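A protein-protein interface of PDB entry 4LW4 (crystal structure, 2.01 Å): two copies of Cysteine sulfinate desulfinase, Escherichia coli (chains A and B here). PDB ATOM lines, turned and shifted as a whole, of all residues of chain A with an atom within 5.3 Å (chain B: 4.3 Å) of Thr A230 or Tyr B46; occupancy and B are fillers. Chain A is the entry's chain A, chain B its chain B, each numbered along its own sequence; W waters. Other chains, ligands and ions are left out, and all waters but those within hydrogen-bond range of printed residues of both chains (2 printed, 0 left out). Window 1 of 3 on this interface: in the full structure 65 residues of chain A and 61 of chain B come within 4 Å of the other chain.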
ATOM      1  N   PRO A  17      15.293  24.003 -21.373  1.00  0.00           N
ATOM      2  CA  PRO A  17      14.228  23.415 -22.137  1.00  0.00           C
ATOM      3  C   PRO A  17      13.172  24.401 -22.651  1.00  0.00           C
ATOM      4  O   PRO A  17      12.488  24.051 -23.603  1.00  0.00           O
ATOM      5  CB  PRO A  17      13.625  22.347 -21.147  1.00  0.00           C
ATOM      6  CG  PRO A  17      13.900  22.932 -19.843  1.00  0.00           C
ATOM      7  CD  PRO A  17      15.351  23.386 -20.020  1.00  0.00           C
ATOM      8  N   LYS A  34      15.241  28.437 -16.700  1.00  0.00           N
ATOM      9  CA  LYS A  34      15.904  27.491 -15.799  1.00  0.00           C
ATOM     10  C   LYS A  34      16.600  26.389 -16.629  1.00  0.00           C
ATOM     11  O   LYS A  34      16.081  25.916 -17.645  1.00  0.00           O
ATOM     12  CB  LYS A  34      14.858  26.740 -14.924  1.00  0.00           C
ATOM     13  CG  LYS A  34      13.757  27.599 -14.268  1.00  0.00           C
ATOM     14  CD  LYS A  34      14.282  28.849 -13.516  1.00  0.00           C
ATOM     15  CE  LYS A  34      13.078  29.756 -13.111  1.00  0.00           C
ATOM     16  NZ  LYS A  34      13.597  31.039 -12.678  1.00  0.00           N
ATOM     17  N   VAL A  38      17.897  22.254 -12.747  1.00  0.00           N
ATOM     18  CA  VAL A  38      16.972  22.815 -11.749  1.00  0.00           C
ATOM     19  C   VAL A  38      15.649  22.116 -11.885  1.00  0.00           C
ATOM     20  O   VAL A  38      15.039  21.741 -10.868  1.00  0.00           O
ATOM     21  CB  VAL A  38      16.787  24.350 -11.903  1.00  0.00           C
ATOM     22  CG1 VAL A  38      15.519  24.851 -11.187  1.00  0.00           C
ATOM     23  CG2 VAL A  38      17.987  25.087 -11.337  1.00  0.00           C
ATOM     24  N   VAL A  39      15.210  21.930 -13.129  1.00  0.00           N
ATOM     25  CA  VAL A  39      13.953  21.223 -13.359  1.00  0.00           C
ATOM     26  C   VAL A  39      14.023  19.795 -12.819  1.00  0.00           C
ATOM     27  O   VAL A  39      13.083  19.248 -12.180  1.00  0.00           O
ATOM     28  CB  VAL A  39      13.614  21.151 -14.877  1.00  0.00           C
ATOM     29  CG1 VAL A  39      12.296  20.385 -15.093  1.00  0.00           C
ATOM     30  CG2 VAL A  39      13.526  22.535 -15.548  1.00  0.00           C
ATOM     31  N   THR A  42      14.180  19.457  -8.941  1.00  0.00           N
ATOM     32  CA  THR A  42      12.871  19.729  -8.394  1.00  0.00           C
ATOM     33  C   THR A  42      11.928  18.528  -8.566  1.00  0.00           C
ATOM     34  O   THR A  42      11.240  18.166  -7.627  1.00  0.00           O
ATOM     35  CB  THR A  42      12.280  21.004  -9.018  1.00  0.00           C
ATOM     36  OG1 THR A  42      13.166  22.122  -8.754  1.00  0.00           O
ATOM     37  CG2 THR A  42      10.790  21.323  -8.461  1.00  0.00           C
ATOM     38  N   HIS A 224      15.229  33.332  -8.290  1.00  0.00           N
ATOM     39  CA  HIS A 224      14.500  33.164  -9.587  1.00  0.00           C
ATOM     40  C   HIS A 224      15.238  33.893 -10.729  1.00  0.00           C
ATOM     41  O   HIS A 224      15.146  33.512 -11.918  1.00  0.00           O
ATOM     42  CB  HIS A 224      13.013  33.558  -9.485  1.00  0.00           C
ATOM     43  CG  HIS A 224      12.790  35.040  -9.262  1.00  0.00           C
ATOM     44  ND1 HIS A 224      12.543  35.933 -10.290  1.00  0.00           N
ATOM     45  CD2 HIS A 224      12.774  35.772  -8.110  1.00  0.00           C
ATOM     46  CE1 HIS A 224      12.370  37.149  -9.777  1.00  0.00           C
ATOM     47  NE2 HIS A 224      12.546  37.077  -8.455  1.00  0.00           N
ATOM     48  N   GLY A 228      17.106  30.153 -11.142  1.00  0.00           N
ATOM     49  CA  GLY A 228      16.717  29.247 -10.056  1.00  0.00           C
ATOM     50  C   GLY A 228      15.216  29.247  -9.678  1.00  0.00           C
ATOM     51  O   GLY A 228      14.407  29.857 -10.371  1.00  0.00           O
ATOM     52  N   PRO A 229      14.850  28.578  -8.560  1.00  0.00           N
ATOM     53  CA  PRO A 229      13.437  28.465  -8.199  1.00  0.00           C
ATOM     54  C   PRO A 229      12.868  29.808  -7.790  1.00  0.00           C
ATOM     55  O   PRO A 229      13.629  30.657  -7.358  1.00  0.00           O
ATOM     56  CB  PRO A 229      13.463  27.455  -6.997  1.00  0.00           C
ATOM     57  CG  PRO A 229      14.756  26.612  -7.304  1.00  0.00           C
ATOM     58  CD  PRO A 229      15.704  27.727  -7.673  1.00  0.00           C
ATOM     59  N   THR A 230      11.545  29.974  -7.874  1.00  0.00           N
ATOM     60  CA  THR A 230      10.844  31.049  -7.152  1.00  0.00           C
ATOM     61  C   THR A 230      10.723  30.743  -5.631  1.00  0.00           C
ATOM     62  O   THR A 230      10.876  29.612  -5.207  1.00  0.00           O
ATOM     63  CB  THR A 230       9.412  31.304  -7.702  1.00  0.00           C
ATOM     64  OG1 THR A 230       8.670  30.083  -7.628  1.00  0.00           O
ATOM     65  CG2 THR A 230       9.487  31.776  -9.200  1.00  0.00           C
ATOM     66  N   GLY A 231      10.442  31.785  -4.858  1.00  0.00           N
ATOM     67  CA  GLY A 231      10.177  31.684  -3.409  1.00  0.00           C
ATOM     68  C   GLY A 231      11.408  31.411  -2.604  1.00  0.00           C
ATOM     69  O   GLY A 231      11.310  30.834  -1.550  1.00  0.00           O
ATOM     70  N   ILE A 232      12.583  31.752  -3.129  1.00  0.00           N
ATOM     71  CA  ILE A 232      13.793  31.485  -2.381  1.00  0.00           C
ATOM     72  C   ILE A 232      14.832  32.614  -2.665  1.00  0.00           C
ATOM     73  O   ILE A 232      14.981  33.083  -3.795  1.00  0.00           O
ATOM     74  CB  ILE A 232      14.419  30.065  -2.722  1.00  0.00           C
ATOM     75  CG1 ILE A 232      15.660  29.804  -1.818  1.00  0.00           C
ATOM     76  CG2 ILE A 232      14.987  30.057  -4.182  1.00  0.00           C
ATOM     77  CD1 ILE A 232      15.361  29.567  -0.345  1.00  0.00           C
ATOM     78  N   ASN A 278      11.675  26.508   2.744  1.00  0.00           N
ATOM     79  CA  ASN A 278      11.355  26.195   1.396  1.00  0.00           C
ATOM     80  C   ASN A 278      12.363  25.187   0.855  1.00  0.00           C
ATOM     81  O   ASN A 278      13.318  25.525   0.119  1.00  0.00           O
ATOM     82  CB  ASN A 278      11.215  27.431   0.521  1.00  0.00           C
ATOM     83  CG  ASN A 278      10.752  27.042  -0.906  1.00  0.00           C
ATOM     84  OD1 ASN A 278      10.504  25.853  -1.171  1.00  0.00           O
ATOM     85  ND2 ASN A 278      10.717  28.003  -1.809  1.00  0.00           N
ATOM     86  N   GLY A 281      12.819  24.996  -2.896  1.00  0.00           N
ATOM     87  CA  GLY A 281      13.534  26.164  -3.368  1.00  0.00           C
ATOM     88  C   GLY A 281      15.030  26.069  -3.000  1.00  0.00           C
ATOM     89  O   GLY A 281      15.863  26.370  -3.828  1.00  0.00           O
ATOM     90  N   THR B  42       4.577  21.640 -11.661  1.00  0.00           N
ATOM     91  CA  THR B  42       5.841  22.267 -11.290  1.00  0.00           C
ATOM     92  C   THR B  42       6.830  22.108 -12.392  1.00  0.00           C
ATOM     93  O   THR B  42       7.526  23.064 -12.791  1.00  0.00           O
ATOM     94  CB  THR B  42       6.359  21.610  -9.984  1.00  0.00           C
ATOM     95  OG1 THR B  42       5.348  21.793  -8.953  1.00  0.00           O
ATOM     96  CG2 THR B  42       7.721  22.223  -9.518  1.00  0.00           C
ATOM     97  N   GLN B  43       6.878  20.899 -12.920  1.00  0.00           N
ATOM     98  CA  GLN B  43       7.789  20.604 -14.040  1.00  0.00           C
ATOM     99  C   GLN B  43       7.481  21.495 -15.229  1.00  0.00           C
ATOM    100  O   GLN B  43       8.365  22.037 -15.839  1.00  0.00           O
ATOM    101  CB  GLN B  43       7.725  19.130 -14.461  1.00  0.00           C
ATOM    102  CG  GLN B  43       8.833  18.788 -15.408  1.00  0.00           C
ATOM    103  CD  GLN B  43       9.016  17.315 -15.606  1.00  0.00           C
ATOM    104  OE1 GLN B  43       8.117  16.632 -16.089  1.00  0.00           O
ATOM    105  NE2 GLN B  43      10.203  16.809 -15.260  1.00  0.00           N
ATOM    106  N   GLN B  44       6.193  21.664 -15.533  1.00  0.00           N
ATOM    107  CA  GLN B  44       5.783  22.534 -16.629  1.00  0.00           C
ATOM    108  C   GLN B  44       6.166  23.980 -16.354  1.00  0.00           C
ATOM    109  O   GLN B  44       6.741  24.616 -17.235  1.00  0.00           O
ATOM    110  CB  GLN B  44       4.258  22.464 -16.906  1.00  0.00           C
ATOM    111  CG  GLN B  44       3.841  21.088 -17.486  1.00  0.00           C
ATOM    112  CD  GLN B  44       4.233  20.999 -18.958  1.00  0.00           C
ATOM    113  OE1 GLN B  44       3.683  21.704 -19.792  1.00  0.00           O
ATOM    114  NE2 GLN B  44       5.234  20.174 -19.268  1.00  0.00           N
ATOM    115  N   PHE B  45       5.884  24.477 -15.137  1.00  0.00           N
ATOM    116  CA  PHE B  45       6.188  25.873 -14.807  1.00  0.00           C
ATOM    117  C   PHE B  45       7.675  26.170 -14.982  1.00  0.00           C
ATOM    118  O   PHE B  45       8.043  27.232 -15.461  1.00  0.00           O
ATOM    119  CB  PHE B  45       5.808  26.196 -13.386  1.00  0.00           C
ATOM    120  CG  PHE B  45       6.239  27.555 -12.955  1.00  0.00           C
ATOM    121  CD1 PHE B  45       5.643  28.683 -13.497  1.00  0.00           C
ATOM    122  CD2 PHE B  45       7.312  27.696 -12.068  1.00  0.00           C
ATOM    123  CE1 PHE B  45       6.080  29.944 -13.129  1.00  0.00           C
ATOM    124  CE2 PHE B  45       7.772  28.947 -11.657  1.00  0.00           C
ATOM    125  CZ  PHE B  45       7.153  30.078 -12.165  1.00  0.00           C
ATOM    126  N   TYR B  46       8.524  25.261 -14.534  1.00  0.00           N
ATOM    127  CA  TYR B  46       9.948  25.502 -14.713  1.00  0.00           C
ATOM    128  C   TYR B  46      10.528  25.191 -16.103  1.00  0.00           C
ATOM    129  O   TYR B  46      11.738  25.449 -16.317  1.00  0.00           O
ATOM    130  CB  TYR B  46      10.757  24.783 -13.682  1.00  0.00           C
ATOM    131  CG  TYR B  46      10.654  25.386 -12.311  1.00  0.00           C
ATOM    132  CD1 TYR B  46      10.770  26.745 -12.117  1.00  0.00           C
ATOM    133  CD2 TYR B  46      10.400  24.565 -11.202  1.00  0.00           C
ATOM    134  CE1 TYR B  46      10.765  27.300 -10.835  1.00  0.00           C
ATOM    135  CE2 TYR B  46      10.340  25.105  -9.919  1.00  0.00           C
ATOM    136  CZ  TYR B  46      10.530  26.484  -9.747  1.00  0.00           C
ATOM    137  OH  TYR B  46      10.396  27.049  -8.490  1.00  0.00           O
ATOM    138  N   SER B  47       9.695  24.697 -17.047  1.00  0.00           N
ATOM    139  CA  SER B  47      10.202  24.246 -18.362  1.00  0.00           C
ATOM    140  C   SER B  47       9.696  25.129 -19.482  1.00  0.00           C
ATOM    141  O   SER B  47      10.001  24.851 -20.634  1.00  0.00           O
ATOM    142  CB  SER B  47       9.745  22.795 -18.672  1.00  0.00           C
ATOM    143  OG  SER B  47      10.449  21.953 -17.759  1.00  0.00           O
ATOM    144  N   LEU B  48       8.897  26.144 -19.132  1.00  0.00           N
ATOM    145  CA  LEU B  48       8.300  27.063 -20.072  1.00  0.00           C
ATOM    146  C   LEU B  48       8.552  28.502 -19.630  1.00  0.00           C
ATOM    147  O   LEU B  48       8.563  28.803 -18.430  1.00  0.00           O
ATOM    148  CB  LEU B  48       6.751  26.870 -20.114  1.00  0.00           C
ATOM    149  CG  LEU B  48       6.280  25.565 -20.769  1.00  0.00           C
ATOM    150  CD1 LEU B  48       4.812  25.298 -20.576  1.00  0.00           C
ATOM    151  CD2 LEU B  48       6.635  25.528 -22.257  1.00  0.00           C
ATOM    152  N   PRO B 277       6.148  36.942  -6.084  1.00  0.00           N
ATOM    153  CA  PRO B 277       5.490  35.813  -5.423  1.00  0.00           C
ATOM    154  C   PRO B 277       6.289  34.532  -5.636  1.00  0.00           C
ATOM    155  O   PRO B 277       7.077  34.425  -6.607  1.00  0.00           O
ATOM    156  CB  PRO B 277       4.146  35.648  -6.211  1.00  0.00           C
ATOM    157  CG  PRO B 277       3.809  36.918  -6.755  1.00  0.00           C
ATOM    158  CD  PRO B 277       5.279  37.518  -7.135  1.00  0.00           C
ATOM    159  N   ASN B 278       6.012  33.550  -4.786  1.00  0.00           N
ATOM    160  CA  ASN B 278       6.546  32.218  -5.034  1.00  0.00           C
ATOM    161  C   ASN B 278       5.609  31.664  -6.083  1.00  0.00           C
ATOM    162  O   ASN B 278       4.684  30.910  -5.775  1.00  0.00           O
ATOM    163  CB  ASN B 278       6.578  31.317  -3.750  1.00  0.00           C
ATOM    164  CG  ASN B 278       7.064  29.916  -4.065  1.00  0.00           C
ATOM    165  OD1 ASN B 278       7.433  29.643  -5.220  1.00  0.00           O
ATOM    166  ND2 ASN B 278       7.023  29.017  -3.087  1.00  0.00           N
ATOM    167  N   VAL B 279       5.848  32.027  -7.339  1.00  0.00           N
ATOM    168  CA  VAL B 279       4.902  31.632  -8.380  1.00  0.00           C
ATOM    169  C   VAL B 279       4.839  30.103  -8.514  1.00  0.00           C
ATOM    170  O   VAL B 279       3.726  29.574  -8.710  1.00  0.00           O
ATOM    171  CB  VAL B 279       5.248  32.232  -9.730  1.00  0.00           C
ATOM    172  CG1 VAL B 279       4.262  31.794 -10.876  1.00  0.00           C
ATOM    173  CG2 VAL B 279       5.229  33.879  -9.652  1.00  0.00           C
ATOM    174  N   ALA B 280       5.994  29.399  -8.470  1.00  0.00           N
ATOM    175  CA  ALA B 280       5.922  27.887  -8.516  1.00  0.00           C
ATOM    176  C   ALA B 280       5.017  27.323  -7.407  1.00  0.00           C
ATOM    177  O   ALA B 280       4.294  26.276  -7.598  1.00  0.00           O
ATOM    178  CB  ALA B 280       7.322  27.244  -8.347  1.00  0.00           C
HETATM  179  O   HOH W   1       9.914  34.348  -6.151  1.00  0.00           O
HETATM  180  O   HOH W   2      12.620  27.643 -17.834  1.00  0.00           O
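The backbone NH (N) of Thr A230 lies within hydrogen-bond range of the side-chain hydroxyl (OH) of Tyr B46, 3.2 Å away. The side-chain hydroxyl (OG1) of Thr A230 is in hydrogen-bond range of the side-chain amide oxygen (OD1) of Asn B278 (2.7 Å). The side-chain hydroxyl (OG1) of Thr A230 sits at hydrogen-bond distance from the backbone NH (N) of Val B279. The backbone NH of Ala B280 sits at hydrogen-bond distance from the side-chain hydroxyl of Thr A230 (2.9 Å).
The side-chain amino group (NZ) of Lys A34 sits at hydrogen-bond distance from the backbone carbonyl oxygen (O) of His A224 (3.0 Å). The side-chain amino group of Lys A34 lies within hydrogen-bond range of the backbone carbonyl oxygen of Gly A228 (2.7 Å). The side-chain hydroxyl of Thr A42 sits at hydrogen-bond distance from the backbone carbonyl oxygen of Val A38, 2.8 Å away. N of His A224 lies within hydrogen-bond range of O of Pro A229 (3.3 Å). The backbone carbonyl oxygen of Gly A231 lies within hydrogen-bond range of the side-chain amide nitrogen of Asn A278. The backbone carbonyl oxygen (O) of Gln B43 is in hydrogen-bond range of the side-chain hydroxyl (OG) of Ser B47 (2.8 Å).
Of the 13 printed residues of chain A, 7 touch a printed residue of chain B. Printed residues of chain A that touch a printed residue of chain B: Pro A17, Lys A34, Val A39, Thr A42, Pro A229, Thr A230 and Gly A231. Along chain A the printed residues that touch a printed residue of chain B span positions 17 to 231. Hydrophobic or aromatic side chains of chain B within 4 Å of the printed part of chain A: Tyr B46 and Ala B280. Among the printed residues, no Asp or Glu carboxylate lies within 4 Å of a Lys or Arg side-chain nitrogen of the other chain.
Printed residues of chain B within 4 Å of Pro A17: Ser B47. Of the printed residues of chain B, Lys A34 touches Tyr B46 (3.6 Å). Printed residues of chain B within 4 Å of Thr A230: Tyr B46 (3.2 Å), Asn B278 (2.7 Å), Val B279 (3.4 Å) and Ala B280 (2.9 Å). Of the printed residues of chain B, Gly A231 touches Asn B278. Of the printed residues of chain A, Thr B42 touches Thr A42. Printed residues of chain A within 4 Å of Gln B43: Val A39 (3.8 Å). Of chain A, only Lys A34 (3.6 Å), Val A39 (3.5 Å), Pro A229 (3.4 Å) and Thr A230 (3.2 Å) come within 4 Å of Tyr B46.
Thr A42 touches its own counterpart, Thr B42. Positions printed for both chains: 42 and 278. Of the 12 pairs that touch across the chains among the printed residues, 1 has its exchanged pair printed and touching as well.
Among the printed residues, pairs that only touch across the chains: Pro A17 with Ser B47, Lys A34 with Tyr B46, Val A39 with Gln B43, Val A39 with Tyr B46, Val A39 with Ser B47, Thr A42 with Thr B42, Pro A229 with Tyr B46 and Gly A231 with Asn B278.
Water W2 bridges O of Tyr B46 (2.8 Å) and N of Lys A34 (3.0 Å). Water W1 bridges the backbone carbonyl oxygen of Pro B277 (2.9 Å) and the backbone NH of Gly A231 (2.9 Å).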
